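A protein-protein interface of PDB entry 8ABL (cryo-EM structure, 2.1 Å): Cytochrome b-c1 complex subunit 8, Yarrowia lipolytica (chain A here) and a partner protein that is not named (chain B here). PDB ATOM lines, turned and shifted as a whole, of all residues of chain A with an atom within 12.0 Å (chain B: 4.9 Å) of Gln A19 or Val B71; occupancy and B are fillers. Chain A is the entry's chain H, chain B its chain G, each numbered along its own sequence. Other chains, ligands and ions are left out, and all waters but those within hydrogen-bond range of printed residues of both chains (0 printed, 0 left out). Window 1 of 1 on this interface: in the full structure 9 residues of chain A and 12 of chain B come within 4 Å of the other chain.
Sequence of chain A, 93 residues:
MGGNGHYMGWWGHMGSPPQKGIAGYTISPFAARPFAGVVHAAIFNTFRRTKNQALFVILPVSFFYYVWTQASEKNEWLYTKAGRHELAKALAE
The side-chain hydroxyl (OG) of Ser A16 sits at hydrogen-bond distance from the side-chain amide nitrogen (NE2) of Gln A19, 3.0 Å away.
Among the printed residues, merely in contact across the chains: Pro A17 with Ser B67, Pro A17 with Arg B70, Pro A17 with Val B71, Pro A18 with Tyr B68, Pro A18 with Val B71, Gln A19 with Val B71, Gln A19 with Ile B75, Lys A20 with Tyr B68, Ile A22 with Val B71, Ile A22 with Tyr B72 and Ile A22 with Ile B75.
Trp A11 touches none of the printed residues of chain B. Gln A19 touches two residues of chain B. Of the printed residues of chain B, Lys A20 touches Tyr B68 (3.5 Å). Ser B67 touches just one residue of chain A: Pro A17 (3.9 Å). Of chain A, only Pro A18 and Lys A20 come within 4 Å of Tyr B68. Of chain A, only Pro A17 comes within 4 Å of Arg B70. Of the printed residues of chain A, Val B71 touches Pro A17, Pro A18, Gln A19 and Ile A22. Printed residues of chain A within 4 Å of Tyr B72: Ile A22 (3.9 Å). Arg B73 touches none of the printed residues of chain A. Ile B75 touches two residues of chain A. The nearest printed residue of chain A that does not touch Val B71 is Ser A16 (4.8 Å). The nearest printed residue of chain B that does not touch Ile A22 is Tyr B68 (5.2 Å).
Among the printed residues, 11 pairs touch across the chains. Among the printed residues, no Asp or Glu carboxylate lies within 4 Å of a Lys or Arg side-chain nitrogen of the other chain.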
ATOM      1  N   GLY A   9     -14.175  18.973   2.896  1.00  0.00           N
ATOM      2  CA  GLY A   9     -13.003  19.272   2.094  1.00  0.00           C
ATOM      3  C   GLY A   9     -12.300  20.500   2.655  1.00  0.00           C
ATOM      4  O   GLY A   9     -11.953  20.534   3.832  1.00  0.00           O
ATOM      5  N   TRP A  10     -12.109  21.506   1.802  1.00  0.00           N
ATOM      6  CA  TRP A  10     -11.443  22.734   2.203  1.00  0.00           C
ATOM      7  C   TRP A  10     -12.012  23.873   1.367  1.00  0.00           C
ATOM      8  O   TRP A  10     -12.821  23.629   0.481  1.00  0.00           O
ATOM      9  CB  TRP A  10      -9.926  22.595   2.030  1.00  0.00           C
ATOM     10  CG  TRP A  10      -9.164  23.525   2.926  1.00  0.00           C
ATOM     11  CD1 TRP A  10      -8.472  24.648   2.569  1.00  0.00           C
ATOM     12  CD2 TRP A  10      -9.052  23.425   4.360  1.00  0.00           C
ATOM     13  NE1 TRP A  10      -7.932  25.249   3.679  1.00  0.00           N
ATOM     14  CE2 TRP A  10      -8.258  24.516   4.792  1.00  0.00           C
ATOM     15  CE3 TRP A  10      -9.535  22.512   5.313  1.00  0.00           C
ATOM     16  CZ2 TRP A  10      -7.932  24.707   6.139  1.00  0.00           C
ATOM     17  CZ3 TRP A  10      -9.198  22.692   6.643  1.00  0.00           C
ATOM     18  CH2 TRP A  10      -8.409  23.779   7.047  1.00  0.00           C
ATOM     19  N   TRP A  11     -11.595  25.114   1.621  1.00  0.00           N
ATOM     20  CA  TRP A  11     -12.144  26.226   0.858  1.00  0.00           C
ATOM     21  C   TRP A  11     -12.038  25.991  -0.651  1.00  0.00           C
ATOM     22  O   TRP A  11     -10.971  25.660  -1.157  1.00  0.00           O
ATOM     23  CB  TRP A  11     -11.426  27.498   1.267  1.00  0.00           C
ATOM     24  CG  TRP A  11     -11.590  27.780   2.726  1.00  0.00           C
ATOM     25  CD1 TRP A  11     -10.653  27.603   3.705  1.00  0.00           C
ATOM     26  CD2 TRP A  11     -12.779  28.282   3.372  1.00  0.00           C
ATOM     27  NE1 TRP A  11     -11.171  27.987   4.916  1.00  0.00           N
ATOM     28  CE2 TRP A  11     -12.470  28.410   4.746  1.00  0.00           C
ATOM     29  CE3 TRP A  11     -14.063  28.651   2.929  1.00  0.00           C
ATOM     30  CZ2 TRP A  11     -13.407  28.889   5.674  1.00  0.00           C
ATOM     31  CZ3 TRP A  11     -14.988  29.129   3.843  1.00  0.00           C
ATOM     32  CH2 TRP A  11     -14.659  29.241   5.201  1.00  0.00           C
ATOM     33  N   GLY A  12     -13.154  26.155  -1.370  1.00  0.00           N
ATOM     34  CA  GLY A  12     -13.153  25.928  -2.805  1.00  0.00           C
ATOM     35  C   GLY A  12     -13.672  24.540  -3.177  1.00  0.00           C
ATOM     36  O   GLY A  12     -14.186  24.364  -4.276  1.00  0.00           O
ATOM     37  N   HIS A  13     -13.569  23.569  -2.268  1.00  0.00           N
ATOM     38  CA  HIS A  13     -14.105  22.239  -2.511  1.00  0.00           C
ATOM     39  C   HIS A  13     -14.582  21.678  -1.181  1.00  0.00           C
ATOM     40  O   HIS A  13     -14.091  20.650  -0.726  1.00  0.00           O
ATOM     41  CB  HIS A  13     -13.053  21.343  -3.193  1.00  0.00           C
ATOM     42  CG  HIS A  13     -11.752  21.280  -2.460  1.00  0.00           C
ATOM     43  ND1 HIS A  13     -10.831  22.303  -2.514  1.00  0.00           N
ATOM     44  CD2 HIS A  13     -11.222  20.336  -1.645  1.00  0.00           C
ATOM     45  CE1 HIS A  13      -9.784  21.992  -1.772  1.00  0.00           C
ATOM     46  NE2 HIS A  13     -10.009  20.793  -1.211  1.00  0.00           N
ATOM     47  N   MET A  14     -15.518  22.381  -0.542  1.00  0.00           N
ATOM     48  CA  MET A  14     -15.882  22.031   0.822  1.00  0.00           C
ATOM     49  C   MET A  14     -16.664  20.714   0.873  1.00  0.00           C
ATOM     50  O   MET A  14     -16.649  20.043   1.899  1.00  0.00           O
ATOM     51  CB  MET A  14     -16.673  23.147   1.514  1.00  0.00           C
ATOM     52  CG  MET A  14     -16.666  23.053   3.037  1.00  0.00           C
ATOM     53  SD  MET A  14     -15.023  23.364   3.745  1.00  0.00           S
ATOM     54  CE  MET A  14     -14.830  25.103   3.349  1.00  0.00           C
ATOM     55  N   GLY A  15     -17.297  20.319  -0.240  1.00  0.00           N
ATOM     56  CA  GLY A  15     -18.119  19.115  -0.282  1.00  0.00           C
ATOM     57  C   GLY A  15     -19.622  19.407  -0.255  1.00  0.00           C
ATOM     58  O   GLY A  15     -20.435  18.491  -0.130  1.00  0.00           O
ATOM     59  N   SER A  16     -19.986  20.683  -0.417  1.00  0.00           N
ATOM     60  CA  SER A  16     -21.363  21.114  -0.584  1.00  0.00           C
ATOM     61  C   SER A  16     -21.934  20.517  -1.866  1.00  0.00           C
ATOM     62  O   SER A  16     -21.233  20.429  -2.868  1.00  0.00           O
ATOM     63  CB  SER A  16     -21.389  22.610  -0.641  1.00  0.00           C
ATOM     64  OG  SER A  16     -22.670  23.100  -1.001  1.00  0.00           O
ATOM     65  N   PRO A  17     -23.231  20.148  -1.919  1.00  0.00           N
ATOM     66  CA  PRO A  17     -23.895  19.967  -3.209  1.00  0.00           C
ATOM     67  C   PRO A  17     -23.768  21.299  -3.941  1.00  0.00           C
ATOM     68  O   PRO A  17     -23.620  22.345  -3.310  1.00  0.00           O
ATOM     69  CB  PRO A  17     -25.368  19.767  -2.841  1.00  0.00           C
ATOM     70  CG  PRO A  17     -25.315  19.270  -1.419  1.00  0.00           C
ATOM     71  CD  PRO A  17     -24.141  19.977  -0.778  1.00  0.00           C
ATOM     72  N   PRO A  18     -23.804  21.309  -5.289  1.00  0.00           N
ATOM     73  CA  PRO A  18     -23.705  22.554  -6.049  1.00  0.00           C
ATOM     74  C   PRO A  18     -24.716  23.585  -5.561  1.00  0.00           C
ATOM     75  O   PRO A  18     -25.869  23.261  -5.301  1.00  0.00           O
ATOM     76  CB  PRO A  18     -24.116  22.135  -7.459  1.00  0.00           C
ATOM     77  CG  PRO A  18     -23.739  20.678  -7.532  1.00  0.00           C
ATOM     78  CD  PRO A  18     -23.950  20.121  -6.144  1.00  0.00           C
ATOM     79  N   GLN A  19     -24.250  24.817  -5.400  1.00  0.00           N
ATOM     80  CA  GLN A  19     -25.144  25.875  -4.973  1.00  0.00           C
ATOM     81  C   GLN A  19     -25.445  26.766  -6.167  1.00  0.00           C
ATOM     82  O   GLN A  19     -24.561  27.079  -6.964  1.00  0.00           O
ATOM     83  CB  GLN A  19     -24.519  26.677  -3.834  1.00  0.00           C
ATOM     84  CG  GLN A  19     -24.069  25.813  -2.659  1.00  0.00           C
ATOM     85  CD  GLN A  19     -23.760  26.622  -1.418  1.00  0.00           C
ATOM     86  OE1 GLN A  19     -24.002  27.827  -1.360  1.00  0.00           O
ATOM     87  NE2 GLN A  19     -23.232  25.961  -0.401  1.00  0.00           N
ATOM     88  N   LYS A  20     -26.706  27.165  -6.279  1.00  0.00           N
ATOM     89  CA  LYS A  20     -27.089  28.053  -7.350  1.00  0.00           C
ATOM     90  C   LYS A  20     -28.392  28.729  -6.970  1.00  0.00           C
ATOM     91  O   LYS A  20     -29.246  28.106  -6.359  1.00  0.00           O
ATOM     92  CB  LYS A  20     -27.301  27.228  -8.615  1.00  0.00           C
ATOM     93  CG  LYS A  20     -27.438  28.084  -9.851  1.00  0.00           C
ATOM     94  CD  LYS A  20     -27.551  27.273 -11.109  1.00  0.00           C
ATOM     95  CE  LYS A  20     -27.698  28.176 -12.314  1.00  0.00           C
ATOM     96  NZ  LYS A  20     -27.799  27.391 -13.566  1.00  0.00           N
ATOM     97  N   GLY A  21     -28.543  29.993  -7.357  1.00  0.00           N
ATOM     98  CA  GLY A  21     -29.814  30.673  -7.209  1.00  0.00           C
ATOM     99  C   GLY A  21     -29.952  31.415  -5.884  1.00  0.00           C
ATOM    100  O   GLY A  21     -30.964  32.068  -5.666  1.00  0.00           O
ATOM    101  N   ILE A  22     -28.956  31.328  -5.000  1.00  0.00           N
ATOM    102  CA  ILE A  22     -29.068  32.024  -3.723  1.00  0.00           C
ATOM    103  C   ILE A  22     -28.245  33.306  -3.799  1.00  0.00           C
ATOM    104  O   ILE A  22     -27.062  33.231  -4.089  1.00  0.00           O
ATOM    105  CB  ILE A  22     -28.540  31.143  -2.571  1.00  0.00           C
ATOM    106  CG1 ILE A  22     -29.241  29.781  -2.492  1.00  0.00           C
ATOM    107  CG2 ILE A  22     -28.594  31.899  -1.245  1.00  0.00           C
ATOM    108  CD1 ILE A  22     -28.498  28.752  -1.655  1.00  0.00           C
ATOM    109  N   ALA A  23     -28.824  34.463  -3.466  1.00  0.00           N
ATOM    110  CA  ALA A  23     -28.014  35.665  -3.385  1.00  0.00           C
ATOM    111  C   ALA A  23     -27.869  36.019  -1.909  1.00  0.00           C
ATOM    112  O   ALA A  23     -28.878  36.102  -1.219  1.00  0.00           O
ATOM    113  CB  ALA A  23     -28.693  36.768  -4.163  1.00  0.00           C
ATOM    114  N   GLY A  24     -26.640  36.222  -1.420  1.00  0.00           N
ATOM    115  CA  GLY A  24     -26.464  36.618  -0.032  1.00  0.00           C
ATOM    116  C   GLY A  24     -25.997  38.063   0.061  1.00  0.00           C
ATOM    117  O   GLY A  24     -25.205  38.497  -0.765  1.00  0.00           O
ATOM    118  N   TYR A  25     -26.479  38.790   1.065  1.00  0.00           N
ATOM    119  CA  TYR A  25     -26.144  40.194   1.203  1.00  0.00           C
ATOM    120  C   TYR A  25     -25.740  40.430   2.640  1.00  0.00           C
ATOM    121  O   TYR A  25     -26.297  39.804   3.535  1.00  0.00           O
ATOM    122  CB  TYR A  25     -27.382  41.054   0.960  1.00  0.00           C
ATOM    123  CG  TYR A  25     -28.012  40.808  -0.384  1.00  0.00           C
ATOM    124  CD1 TYR A  25     -28.829  39.702  -0.613  1.00  0.00           C
ATOM    125  CD2 TYR A  25     -27.780  41.679  -1.440  1.00  0.00           C
ATOM    126  CE1 TYR A  25     -29.410  39.477  -1.854  1.00  0.00           C
ATOM    127  CE2 TYR A  25     -28.346  41.466  -2.688  1.00  0.00           C
ATOM    128  CZ  TYR A  25     -29.162  40.365  -2.890  1.00  0.00           C
ATOM    129  OH  TYR A  25     -29.705  40.159  -4.120  1.00  0.00           O
ATOM    130  N   SER B  67     -32.229  19.303  -5.238  1.00  0.00           N
ATOM    131  CA  SER B  67     -30.932  19.452  -4.620  1.00  0.00           C
ATOM    132  C   SER B  67     -30.654  20.926  -4.320  1.00  0.00           C
ATOM    133  O   SER B  67     -30.171  21.243  -3.240  1.00  0.00           O
ATOM    134  CB  SER B  67     -29.898  18.848  -5.492  1.00  0.00           C
ATOM    135  OG  SER B  67     -28.616  19.037  -4.926  1.00  0.00           O
ATOM    136  N   TYR B  68     -31.005  21.830  -5.241  1.00  0.00           N
ATOM    137  CA  TYR B  68     -30.729  23.238  -4.999  1.00  0.00           C
ATOM    138  C   TYR B  68     -31.633  23.763  -3.897  1.00  0.00           C
ATOM    139  O   TYR B  68     -31.216  24.621  -3.132  1.00  0.00           O
ATOM    140  CB  TYR B  68     -30.983  24.106  -6.228  1.00  0.00           C
ATOM    141  CG  TYR B  68     -30.017  23.889  -7.354  1.00  0.00           C
ATOM    142  CD1 TYR B  68     -28.648  23.933  -7.144  1.00  0.00           C
ATOM    143  CD2 TYR B  68     -30.475  23.663  -8.646  1.00  0.00           C
ATOM    144  CE1 TYR B  68     -27.754  23.737  -8.186  1.00  0.00           C
ATOM    145  CE2 TYR B  68     -29.594  23.460  -9.699  1.00  0.00           C
ATOM    146  CZ  TYR B  68     -28.230  23.508  -9.470  1.00  0.00           C
ATOM    147  OH  TYR B  68     -27.355  23.313 -10.502  1.00  0.00           O
ATOM    148  N   ASP B  69     -32.868  23.265  -3.822  1.00  0.00           N
ATOM    149  CA  ASP B  69     -33.765  23.771  -2.796  1.00  0.00           C
ATOM    150  C   ASP B  69     -33.337  23.278  -1.417  1.00  0.00           C
ATOM    151  O   ASP B  69     -33.524  23.967  -0.421  1.00  0.00           O
ATOM    152  CB  ASP B  69     -35.199  23.311  -3.017  1.00  0.00           C
ATOM    153  CG  ASP B  69     -35.850  23.854  -4.277  1.00  0.00           C
ATOM    154  OD1 ASP B  69     -35.270  24.750  -4.936  1.00  0.00           O
ATOM    155  OD2 ASP B  69     -36.958  23.383  -4.594  1.00  0.00           O
ATOM    156  N   ARG B  70     -32.799  22.062  -1.349  1.00  0.00           N
ATOM    157  CA  ARG B  70     -32.339  21.544  -0.079  1.00  0.00           C
ATOM    158  C   ARG B  70     -31.167  22.398   0.401  1.00  0.00           C
ATOM    159  O   ARG B  70     -31.125  22.787   1.561  1.00  0.00           O
ATOM    160  CB  ARG B  70     -31.916  20.095  -0.284  1.00  0.00           C
ATOM    161  CG  ARG B  70     -31.267  19.467   0.943  1.00  0.00           C
ATOM    162  CD  ARG B  70     -30.942  17.986   0.821  1.00  0.00           C
ATOM    163  NE  ARG B  70     -30.153  17.460   1.930  1.00  0.00           N
ATOM    164  CZ  ARG B  70     -28.831  17.544   2.057  1.00  0.00           C
ATOM    165  NH1 ARG B  70     -28.243  17.000   3.106  1.00  0.00           N
ATOM    166  NH2 ARG B  70     -28.094  18.162   1.150  1.00  0.00           N
ATOM    167  N   VAL B  71     -30.225  22.709  -0.494  1.00  0.00           N
ATOM    168  CA  VAL B  71     -29.128  23.580  -0.112  1.00  0.00           C
ATOM    169  C   VAL B  71     -29.665  24.874   0.492  1.00  0.00           C
ATOM    170  O   VAL B  71     -29.179  25.328   1.518  1.00  0.00           O
ATOM    171  CB  VAL B  71     -28.194  23.879  -1.297  1.00  0.00           C
ATOM    172  CG1 VAL B  71     -27.294  25.077  -1.028  1.00  0.00           C
ATOM    173  CG2 VAL B  71     -27.373  22.652  -1.651  1.00  0.00           C
ATOM    174  N   TYR B  72     -30.650  25.488  -0.153  1.00  0.00           N
ATOM    175  CA  TYR B  72     -31.157  26.739   0.381  1.00  0.00           C
ATOM    176  C   TYR B  72     -31.782  26.553   1.762  1.00  0.00           C
ATOM    177  O   TYR B  72     -31.577  27.395   2.634  1.00  0.00           O
ATOM    178  CB  TYR B  72     -32.211  27.365  -0.527  1.00  0.00           C
ATOM    179  CG  TYR B  72     -32.830  28.601   0.079  1.00  0.00           C
ATOM    180  CD1 TYR B  72     -32.033  29.696   0.367  1.00  0.00           C
ATOM    181  CD2 TYR B  72     -34.179  28.672   0.412  1.00  0.00           C
ATOM    182  CE1 TYR B  72     -32.557  30.844   0.937  1.00  0.00           C
ATOM    183  CE2 TYR B  72     -34.717  29.802   1.016  1.00  0.00           C
ATOM    184  CZ  TYR B  72     -33.904  30.900   1.247  1.00  0.00           C
ATOM    185  OH  TYR B  72     -34.397  32.047   1.798  1.00  0.00           O
ATOM    186  N   ARG B  73     -32.577  25.495   1.953  1.00  0.00           N
ATOM    187  CA  ARG B  73     -33.196  25.304   3.258  1.00  0.00           C
ATOM    188  C   ARG B  73     -32.134  25.072   4.333  1.00  0.00           C
ATOM    189  O   ARG B  73     -32.332  25.503   5.451  1.00  0.00           O
ATOM    190  CB  ARG B  73     -34.191  24.138   3.320  1.00  0.00           C
ATOM    191  CG  ARG B  73     -35.469  24.317   2.507  1.00  0.00           C
ATOM    192  CD  ARG B  73     -36.527  23.243   2.778  1.00  0.00           C
ATOM    193  NE  ARG B  73     -35.988  21.915   2.532  1.00  0.00           N
ATOM    194  CZ  ARG B  73     -35.906  21.325   1.341  1.00  0.00           C
ATOM    195  NH1 ARG B  73     -35.326  20.142   1.260  1.00  0.00           N
ATOM    196  NH2 ARG B  73     -36.385  21.909   0.255  1.00  0.00           N
ATOM    197  N   LEU B  74     -31.010  24.416   4.022  1.00  0.00           N
ATOM    198  CA  LEU B  74     -29.995  24.213   5.047  1.00  0.00           C
ATOM    199  C   LEU B  74     -29.337  25.542   5.414  1.00  0.00           C
ATOM    200  O   LEU B  74     -29.050  25.792   6.581  1.00  0.00           O
ATOM    201  CB  LEU B  74     -28.944  23.220   4.545  1.00  0.00           C
ATOM    202  CG  LEU B  74     -29.433  21.798   4.250  1.00  0.00           C
ATOM    203  CD1 LEU B  74     -28.286  20.901   3.782  1.00  0.00           C
ATOM    204  CD2 LEU B  74     -30.144  21.186   5.450  1.00  0.00           C
ATOM    205  N   ILE B  75     -29.090  26.381   4.408  1.00  0.00           N
ATOM    206  CA  ILE B  75     -28.415  27.641   4.642  1.00  0.00           C
ATOM    207  C   ILE B  75     -29.370  28.540   5.415  1.00  0.00           C
ATOM    208  O   ILE B  75     -28.996  29.175   6.381  1.00  0.00           O
ATOM    209  CB  ILE B  75     -27.971  28.265   3.307  1.00  0.00           C
ATOM    210  CG1 ILE B  75     -26.777  27.497   2.734  1.00  0.00           C
ATOM    211  CG2 ILE B  75     -27.670  29.751   3.481  1.00  0.00           C
ATOM    212  CD1 ILE B  75     -26.392  27.881   1.316  1.00  0.00           C
